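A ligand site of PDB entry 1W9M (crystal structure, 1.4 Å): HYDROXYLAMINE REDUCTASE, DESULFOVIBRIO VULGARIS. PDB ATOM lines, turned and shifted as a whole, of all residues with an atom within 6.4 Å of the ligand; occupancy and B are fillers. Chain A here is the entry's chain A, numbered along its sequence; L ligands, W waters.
FE4 of the ligand is bound by OE2 of Glu 494 (2.1 Å).
An iron atom (FE3) of the ligand is bound by a ring nitrogen (NE2) of His 244 (2.1 Å).
The side-chain carboxylate of Glu 268 binds an iron atom (FE3) of the ligand.
SG of Cys 434 is bound to FE1 of the ligand (2.3 Å).
The side-chain sulfur of Cys 312 binds an iron atom (FE2) of the ligand (2.3 Å).
An iron atom (FE3) of the ligand is bound by the side-chain sulfur (SG) of Cys 459, at 2.4 Å.
SD of CSS 406 is bound to an iron atom (FE4) of the ligand, at 2.5 Å.
The side-chain amide nitrogen of Asn 311 sits close to an oxygen (O1) of the ligand (2.7 Å).
A sulfur (S2) of the ligand sits close to the indole nitrogen of Trp 292, at 3.8 Å.
The side-chain carboxylate of Glu 494 sits close to the side-chain amide nitrogen of Asn 311 (2.8 Å).
The side-chain carboxylate (OE1) of Glu 494 lies within hydrogen-bond range of the backbone NH (N) of Lys 496 (3.0 Å).
ND1 of His 244 is in hydrogen-bond range of OG1 of Thr 310 (2.8 Å).
N of Cys 434 lies within hydrogen-bond range of O of Gly 405 (3.2 Å).
NZ of Lys 496 lies within hydrogen-bond range of OD1 of Asn 311, at 2.9 Å.
ND2 of Asn 311 lies within hydrogen-bond range of O of Thr 71 (3.2 Å).
The indole nitrogen (NE1) of Trp 292 sits at hydrogen-bond distance from the backbone carbonyl oxygen (O) of Asp 407, 2.9 Å away.
OH of Tyr 493 sits at hydrogen-bond distance from ND2 of Asn 72.
O3 of the ligand lies close to NZ of Lys 496, 3.0 Å away.
Tyr 493 touches the ligand (CD2 to S2, 3.8 Å).
Hydrophobic or aromatic side chains within 4 Å of the ligand: His 244, Trp 292 and Tyr 493.
11 residues have an atom within 4 Å of the ligand: His 244, Glu 268, Trp 292, Asn 311, Cys 312, CSS 406, Cys 434, Cys 459, Tyr 493, Glu 494 and Lys 496.
Water W1 lies within hydrogen-bond range of N of Glu 268 (2.9 Å), N of Gly 243 (3.3 Å) and S1 of the ligand (3.3 Å).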
ATOM      1  N   ILE A  70     -16.405  22.933  25.556  1.00  0.00           N
ATOM      2  CA  ILE A  70     -16.953  24.269  25.241  1.00  0.00           C
ATOM      3  C   ILE A  70     -17.251  25.046  26.499  1.00  0.00           C
ATOM      4  O   ILE A  70     -17.580  24.485  27.561  1.00  0.00           O
ATOM      5  CB  ILE A  70     -18.219  24.099  24.329  1.00  0.00           C
ATOM      6  CG1 ILE A  70     -17.759  23.749  22.902  1.00  0.00           C
ATOM      7  CG2 ILE A  70     -19.173  25.249  24.337  1.00  0.00           C
ATOM      8  CD1 ILE A  70     -18.910  23.606  21.944  1.00  0.00           C
ATOM      9  N   THR A  71     -17.143  26.361  26.382  1.00  0.00           N
ATOM     10  CA  THR A  71     -17.418  27.227  27.537  1.00  0.00           C
ATOM     11  C   THR A  71     -18.788  26.930  28.173  1.00  0.00           C
ATOM     12  O   THR A  71     -19.824  26.858  27.492  1.00  0.00           O
ATOM     13  CB  THR A  71     -17.396  28.692  27.064  1.00  0.00           C
ATOM     14  OG1 THR A  71     -16.123  28.930  26.410  1.00  0.00           O
ATOM     15  CG2 THR A  71     -17.586  29.635  28.254  1.00  0.00           C
ATOM     16  N   ASN A  72     -18.759  26.769  29.512  1.00  0.00           N
ATOM     17  CA  ASN A  72     -19.942  26.560  30.323  1.00  0.00           C
ATOM     18  C   ASN A  72     -20.687  25.258  30.009  1.00  0.00           C
ATOM     19  O   ASN A  72     -21.878  25.117  30.293  1.00  0.00           O
ATOM     20  CB  ASN A  72     -20.953  27.722  30.204  1.00  0.00           C
ATOM     21  CG  ASN A  72     -20.380  29.068  30.633  1.00  0.00           C
ATOM     22  OD1 ASN A  72     -19.558  29.115  31.556  1.00  0.00           O
ATOM     23  ND2 ASN A  72     -20.833  30.139  29.982  1.00  0.00           N
ATOM     24  N   TYR A 161     -22.848  21.279  16.930  1.00  0.00           N
ATOM     25  CA  TYR A 161     -23.987  21.144  16.014  1.00  0.00           C
ATOM     26  C   TYR A 161     -24.084  19.736  15.440  1.00  0.00           C
ATOM     27  O   TYR A 161     -25.180  19.202  15.247  1.00  0.00           O
ATOM     28  CB  TYR A 161     -23.827  22.182  14.879  1.00  0.00           C
ATOM     29  CG  TYR A 161     -23.924  23.615  15.344  1.00  0.00           C
ATOM     30  CD1 TYR A 161     -24.683  24.016  16.446  1.00  0.00           C
ATOM     31  CD2 TYR A 161     -23.275  24.613  14.606  1.00  0.00           C
ATOM     32  CE1 TYR A 161     -24.757  25.367  16.823  1.00  0.00           C
ATOM     33  CE2 TYR A 161     -23.336  25.969  14.965  1.00  0.00           C
ATOM     34  CZ  TYR A 161     -24.089  26.330  16.087  1.00  0.00           C
ATOM     35  OH  TYR A 161     -24.156  27.670  16.437  1.00  0.00           O
ATOM     36  N   GLY A 243     -30.444  25.243  27.304  1.00  0.00           N
ATOM     37  CA  GLY A 243     -29.489  24.727  26.333  1.00  0.00           C
ATOM     38  C   GLY A 243     -30.105  24.647  24.936  1.00  0.00           C
ATOM     39  O   GLY A 243     -30.826  25.574  24.579  1.00  0.00           O
ATOM     40  N   HIS A 244     -29.817  23.575  24.181  1.00  0.00           N
ATOM     41  CA  HIS A 244     -30.204  23.592  22.743  1.00  0.00           C
ATOM     42  C   HIS A 244     -30.861  22.321  22.250  1.00  0.00           C
ATOM     43  O   HIS A 244     -31.378  22.339  21.117  1.00  0.00           O
ATOM     44  CB  HIS A 244     -28.978  23.812  21.840  1.00  0.00           C
ATOM     45  CG  HIS A 244     -28.227  25.103  22.061  1.00  0.00           C
ATOM     46  ND1 HIS A 244     -27.482  25.357  23.197  1.00  0.00           N
ATOM     47  CD2 HIS A 244     -28.091  26.199  21.268  1.00  0.00           C
ATOM     48  CE1 HIS A 244     -26.948  26.570  23.062  1.00  0.00           C
ATOM     49  NE2 HIS A 244     -27.294  27.113  21.902  1.00  0.00           N
ATOM     50  N   GLY A 267     -33.418  30.347  27.679  1.00  0.00           N
ATOM     51  CA  GLY A 267     -32.179  30.559  26.967  1.00  0.00           C
ATOM     52  C   GLY A 267     -32.311  30.161  25.516  1.00  0.00           C
ATOM     53  O   GLY A 267     -33.174  30.667  24.780  1.00  0.00           O
ATOM     54  N   GLU A 268     -31.452  29.232  25.102  1.00  0.00           N
ATOM     55  CA  GLU A 268     -31.458  28.729  23.714  1.00  0.00           C
ATOM     56  C   GLU A 268     -32.495  27.653  23.468  1.00  0.00           C
ATOM     57  O   GLU A 268     -32.584  27.136  22.351  1.00  0.00           O
ATOM     58  CB  GLU A 268     -30.045  28.340  23.299  1.00  0.00           C
ATOM     59  CG  GLU A 268     -29.246  29.603  22.905  1.00  0.00           C
ATOM     60  CD  GLU A 268     -29.424  29.909  21.411  1.00  0.00           C
ATOM     61  OE1 GLU A 268     -30.501  30.462  21.069  1.00  0.00           O
ATOM     62  OE2 GLU A 268     -28.511  29.540  20.644  1.00  0.00           O
ATOM     63  N   SER A 291     -31.282  35.831  29.258  1.00  0.00           N
ATOM     64  CA  SER A 291     -30.088  35.241  28.715  1.00  0.00           C
ATOM     65  C   SER A 291     -29.375  34.302  29.664  1.00  0.00           C
ATOM     66  O   SER A 291     -29.646  34.322  30.878  1.00  0.00           O
ATOM     67  CB  SER A 291     -29.119  36.421  28.355  1.00  0.00           C
ATOM     68  OG  SER A 291     -28.156  35.864  27.510  1.00  0.00           O
ATOM     69  N   TRP A 292     -28.457  33.469  29.150  1.00  0.00           N
ATOM     70  CA  TRP A 292     -27.846  32.450  30.015  1.00  0.00           C
ATOM     71  C   TRP A 292     -27.170  33.052  31.243  1.00  0.00           C
ATOM     72  O   TRP A 292     -27.171  32.417  32.313  1.00  0.00           O
ATOM     73  CB  TRP A 292     -26.844  31.613  29.215  1.00  0.00           C
ATOM     74  CG  TRP A 292     -25.680  32.396  28.666  1.00  0.00           C
ATOM     75  CD1 TRP A 292     -25.592  32.950  27.396  1.00  0.00           C
ATOM     76  CD2 TRP A 292     -24.422  32.720  29.324  1.00  0.00           C
ATOM     77  NE1 TRP A 292     -24.389  33.594  27.262  1.00  0.00           N
ATOM     78  CE2 TRP A 292     -23.637  33.468  28.405  1.00  0.00           C
ATOM     79  CE3 TRP A 292     -23.922  32.435  30.606  1.00  0.00           C
ATOM     80  CZ2 TRP A 292     -22.372  33.921  28.755  1.00  0.00           C
ATOM     81  CZ3 TRP A 292     -22.653  32.910  30.917  1.00  0.00           C
ATOM     82  CH2 TRP A 292     -21.870  33.647  30.018  1.00  0.00           C
ATOM     83  N   THR A 310     -27.363  21.342  27.253  1.00  0.00           N
ATOM     84  CA  THR A 310     -26.081  21.736  26.707  1.00  0.00           C
ATOM     85  C   THR A 310     -25.581  22.910  27.561  1.00  0.00           C
ATOM     86  O   THR A 310     -26.261  23.288  28.540  1.00  0.00           O
ATOM     87  CB  THR A 310     -26.153  22.268  25.235  1.00  0.00           C
ATOM     88  OG1 THR A 310     -26.935  23.487  25.207  1.00  0.00           O
ATOM     89  CG2 THR A 310     -26.833  21.307  24.280  1.00  0.00           C
ATOM     90  N   ASN A 311     -24.449  23.495  27.141  1.00  0.00           N
ATOM     91  CA  ASN A 311     -24.104  24.812  27.704  1.00  0.00           C
ATOM     92  C   ASN A 311     -25.222  25.835  27.335  1.00  0.00           C
ATOM     93  O   ASN A 311     -26.005  25.604  26.397  1.00  0.00           O
ATOM     94  CB  ASN A 311     -22.742  25.250  27.170  1.00  0.00           C
ATOM     95  CG  ASN A 311     -22.717  25.473  25.666  1.00  0.00           C
ATOM     96  OD1 ASN A 311     -23.256  24.705  24.867  1.00  0.00           O
ATOM     97  ND2 ASN A 311     -22.120  26.576  25.252  1.00  0.00           N
ATOM     98  N   CYS A 312     -25.320  26.958  28.029  1.00  0.00           N
ATOM     99  CA  CYS A 312     -24.427  27.420  29.100  1.00  0.00           C
ATOM    100  C   CYS A 312     -25.001  27.119  30.496  1.00  0.00           C
ATOM    101  O   CYS A 312     -26.123  27.595  30.819  1.00  0.00           O
ATOM    102  CB  CYS A 312     -24.222  28.923  28.994  1.00  0.00           C
ATOM    103  SG  CYS A 312     -23.155  29.333  27.554  1.00  0.00           S
ATOM    104  N   GLY A 405     -26.022  35.829  17.066  1.00  0.00           N
ATOM    105  CA  GLY A 405     -24.815  35.405  17.764  1.00  0.00           C
ATOM    106  C   GLY A 405     -25.139  35.021  19.195  1.00  0.00           C
ATOM    107  O   GLY A 405     -26.230  34.579  19.534  1.00  0.00           O
ATOM    108  N   CSS A 406     -24.128  35.195  20.038  1.00  0.00           N
ATOM    109  CA  CSS A 406     -24.188  34.734  21.423  1.00  0.00           C
ATOM    110  CB  CSS A 406     -23.161  33.572  21.656  1.00  0.00           C
ATOM    111  SG  CSS A 406     -23.556  32.199  20.554  1.00  0.00           S
ATOM    112  SD  CSS A 406     -22.095  30.793  21.209  1.00  0.00           S
ATOM    113  C   CSS A 406     -23.912  35.917  22.347  1.00  0.00           C
ATOM    114  O   CSS A 406     -22.963  36.691  22.119  1.00  0.00           O
ATOM    115  N   ASP A 407     -24.719  36.047  23.377  1.00  0.00           N
ATOM    116  CA  ASP A 407     -24.657  37.048  24.430  1.00  0.00           C
ATOM    117  C   ASP A 407     -23.629  36.681  25.500  1.00  0.00           C
ATOM    118  O   ASP A 407     -23.084  35.563  25.555  1.00  0.00           O
ATOM    119  CB  ASP A 407     -26.045  37.110  25.103  1.00  0.00           C
ATOM    120  CG  ASP A 407     -26.334  38.367  25.882  1.00  0.00           C
ATOM    121  OD1 ASP A 407     -25.679  39.398  25.670  1.00  0.00           O
ATOM    122  OD2 ASP A 407     -27.263  38.340  26.722  1.00  0.00           O
ATOM    123  N   GLY A 433     -29.778  32.845  18.071  1.00  0.00           N
ATOM    124  CA  GLY A 433     -28.814  32.716  19.142  1.00  0.00           C
ATOM    125  C   GLY A 433     -29.118  33.661  20.291  1.00  0.00           C
ATOM    126  O   GLY A 433     -29.900  34.608  20.154  1.00  0.00           O
ATOM    127  N   CYS A 434     -28.469  33.414  21.440  1.00  0.00           N
ATOM    128  CA  CYS A 434     -28.880  34.175  22.642  1.00  0.00           C
ATOM    129  C   CYS A 434     -28.486  35.646  22.573  1.00  0.00           C
ATOM    130  O   CYS A 434     -28.963  36.435  23.420  1.00  0.00           O
ATOM    131  CB  CYS A 434     -28.398  33.482  23.933  1.00  0.00           C
ATOM    132  SG  CYS A 434     -26.582  33.415  24.038  1.00  0.00           S
ATOM    133  N   ALA A 435     -27.729  36.100  21.582  1.00  0.00           N
ATOM    134  CA  ALA A 435     -27.549  37.546  21.360  1.00  0.00           C
ATOM    135  C   ALA A 435     -28.892  38.264  21.271  1.00  0.00           C
ATOM    136  O   ALA A 435     -28.940  39.456  21.604  1.00  0.00           O
ATOM    137  CB  ALA A 435     -26.773  37.782  20.051  1.00  0.00           C
ATOM    138  N   GLN A 458     -32.206  29.348  17.216  1.00  0.00           N
ATOM    139  CA  GLN A 458     -30.987  29.144  18.016  1.00  0.00           C
ATOM    140  C   GLN A 458     -29.776  29.689  17.269  1.00  0.00           C
ATOM    141  O   GLN A 458     -29.917  30.045  16.083  1.00  0.00           O
ATOM    142  CB  GLN A 458     -30.824  27.639  18.250  1.00  0.00           C
ATOM    143  CG  GLN A 458     -32.032  27.061  19.010  1.00  0.00           C
ATOM    144  CD  GLN A 458     -31.913  25.549  19.164  1.00  0.00           C
ATOM    145  OE1 GLN A 458     -31.694  24.812  18.192  1.00  0.00           O
ATOM    146  NE2 GLN A 458     -32.088  25.077  20.404  1.00  0.00           N
ATOM    147  N   CYS A 459     -28.592  29.715  17.874  1.00  0.00           N
ATOM    148  CA  CYS A 459     -27.427  30.184  17.142  1.00  0.00           C
ATOM    149  C   CYS A 459     -27.230  29.384  15.872  1.00  0.00           C
ATOM    150  O   CYS A 459     -26.867  29.955  14.829  1.00  0.00           O
ATOM    151  CB  CYS A 459     -26.186  30.183  18.066  1.00  0.00           C
ATOM    152  SG  CYS A 459     -25.911  28.572  18.857  1.00  0.00           S
ATOM    153  N   ASN A 460     -27.505  28.075  15.893  1.00  0.00           N
ATOM    154  CA  ASN A 460     -27.420  27.285  14.668  1.00  0.00           C
ATOM    155  C   ASN A 460     -28.375  27.752  13.564  1.00  0.00           C
ATOM    156  O   ASN A 460     -28.098  27.508  12.387  1.00  0.00           O
ATOM    157  CB  ASN A 460     -27.699  25.770  14.935  1.00  0.00           C
ATOM    158  CG  ASN A 460     -28.728  25.533  16.033  1.00  0.00           C
ATOM    159  OD1 ASN A 460     -29.875  25.074  15.773  1.00  0.00           O
ATOM    160  ND2 ASN A 460     -28.317  25.829  17.262  1.00  0.00           N
ATOM    161  N   TYR A 493     -19.672  34.809  21.800  1.00  0.00           N
ATOM    162  CA  TYR A 493     -19.284  34.479  23.179  1.00  0.00           C
ATOM    163  C   TYR A 493     -18.425  33.239  23.143  1.00  0.00           C
ATOM    164  O   TYR A 493     -17.236  33.285  23.503  1.00  0.00           O
ATOM    165  CB  TYR A 493     -20.475  34.283  24.099  1.00  0.00           C
ATOM    166  CG  TYR A 493     -20.035  33.791  25.461  1.00  0.00           C
ATOM    167  CD1 TYR A 493     -19.194  34.571  26.266  1.00  0.00           C
ATOM    168  CD2 TYR A 493     -20.474  32.568  25.939  1.00  0.00           C
ATOM    169  CE1 TYR A 493     -18.793  34.104  27.530  1.00  0.00           C
ATOM    170  CE2 TYR A 493     -20.080  32.099  27.191  1.00  0.00           C
ATOM    171  CZ  TYR A 493     -19.239  32.852  28.001  1.00  0.00           C
ATOM    172  OH  TYR A 493     -18.873  32.347  29.251  1.00  0.00           O
ATOM    173  N   GLU A 494     -19.018  32.112  22.694  1.00  0.00           N
ATOM    174  CA  GLU A 494     -18.150  30.887  22.733  1.00  0.00           C
ATOM    175  C   GLU A 494     -17.962  30.315  21.336  1.00  0.00           C
ATOM    176  O   GLU A 494     -17.947  31.052  20.314  1.00  0.00           O
ATOM    177  CB  GLU A 494     -18.663  29.922  23.816  1.00  0.00           C
ATOM    178  CG  GLU A 494     -20.131  29.581  23.866  1.00  0.00           C
ATOM    179  CD  GLU A 494     -20.560  28.410  22.994  1.00  0.00           C
ATOM    180  OE1 GLU A 494     -19.745  27.729  22.323  1.00  0.00           O
ATOM    181  OE2 GLU A 494     -21.805  28.193  23.027  1.00  0.00           O
ATOM    182  N   GLN A 495     -17.687  28.999  21.276  1.00  0.00           N
ATOM    183  CA  GLN A 495     -17.076  28.373  20.117  1.00  0.00           C
ATOM    184  C   GLN A 495     -18.113  28.073  19.024  1.00  0.00           C
ATOM    185  O   GLN A 495     -17.749  28.090  17.825  1.00  0.00           O
ATOM    186  CB  GLN A 495     -16.283  27.120  20.549  1.00  0.00           C
ATOM    187  CG  GLN A 495     -15.205  27.504  21.595  1.00  0.00           C
ATOM    188  CD  GLN A 495     -15.696  27.738  23.011  1.00  0.00           C
ATOM    189  OE1 GLN A 495     -16.485  26.942  23.555  1.00  0.00           O
ATOM    190  NE2 GLN A 495     -15.301  28.868  23.621  1.00  0.00           N
ATOM    191  N   LYS A 496     -19.376  27.859  19.379  1.00  0.00           N
ATOM    192  CA  LYS A 496     -20.428  27.771  18.338  1.00  0.00           C
ATOM    193  C   LYS A 496     -20.484  29.088  17.566  1.00  0.00           C
ATOM    194  O   LYS A 496     -20.607  29.071  16.345  1.00  0.00           O
ATOM    195  CB  LYS A 496     -21.759  27.392  19.000  1.00  0.00           C
ATOM    196  CG  LYS A 496     -21.852  25.867  19.147  1.00  0.00           C
ATOM    197  CD  LYS A 496     -23.137  25.451  19.921  1.00  0.00           C
ATOM    198  CE  LYS A 496     -22.824  25.378  21.403  1.00  0.00           C
ATOM    199  NZ  LYS A 496     -24.089  25.495  22.185  1.00  0.00           N
ATOM    200  N   ALA A 497     -20.436  30.226  18.232  1.00  0.00           N
ATOM    201  CA  ALA A 497     -20.456  31.523  17.508  1.00  0.00           C
ATOM    202  C   ALA A 497     -19.285  31.612  16.553  1.00  0.00           C
ATOM    203  O   ALA A 497     -19.408  32.148  15.447  1.00  0.00           O
ATOM    204  CB  ALA A 497     -20.357  32.686  18.470  1.00  0.00           C
HETATM  205 FE1  LIG L   1     -25.963  31.188  23.937  1.00  0.00          FE
HETATM  206 FE2  LIG L   1     -24.544  29.702  25.701  1.00  0.00          FE
HETATM  207 FE3  LIG L   1     -26.520  28.943  21.157  1.00  0.00          FE
HETATM  208 FE4  LIG L   1     -23.432  29.449  22.790  1.00  0.00          FE
HETATM  209  S1  LIG L   1     -26.711  29.840  25.610  1.00  0.00           S
HETATM  210  S2  LIG L   1     -23.680  31.290  24.355  1.00  0.00           S
HETATM  211  O1  LIG L   1     -24.215  28.090  24.444  1.00  0.00           O
HETATM  212  O2  LIG L   1     -26.258  30.774  21.963  1.00  0.00           O
HETATM  213  O3  LIG L   1     -24.524  28.365  21.613  1.00  0.00           O
HETATM  214  O   HOH W   1     -29.306  28.256  26.830  1.00  0.00           O
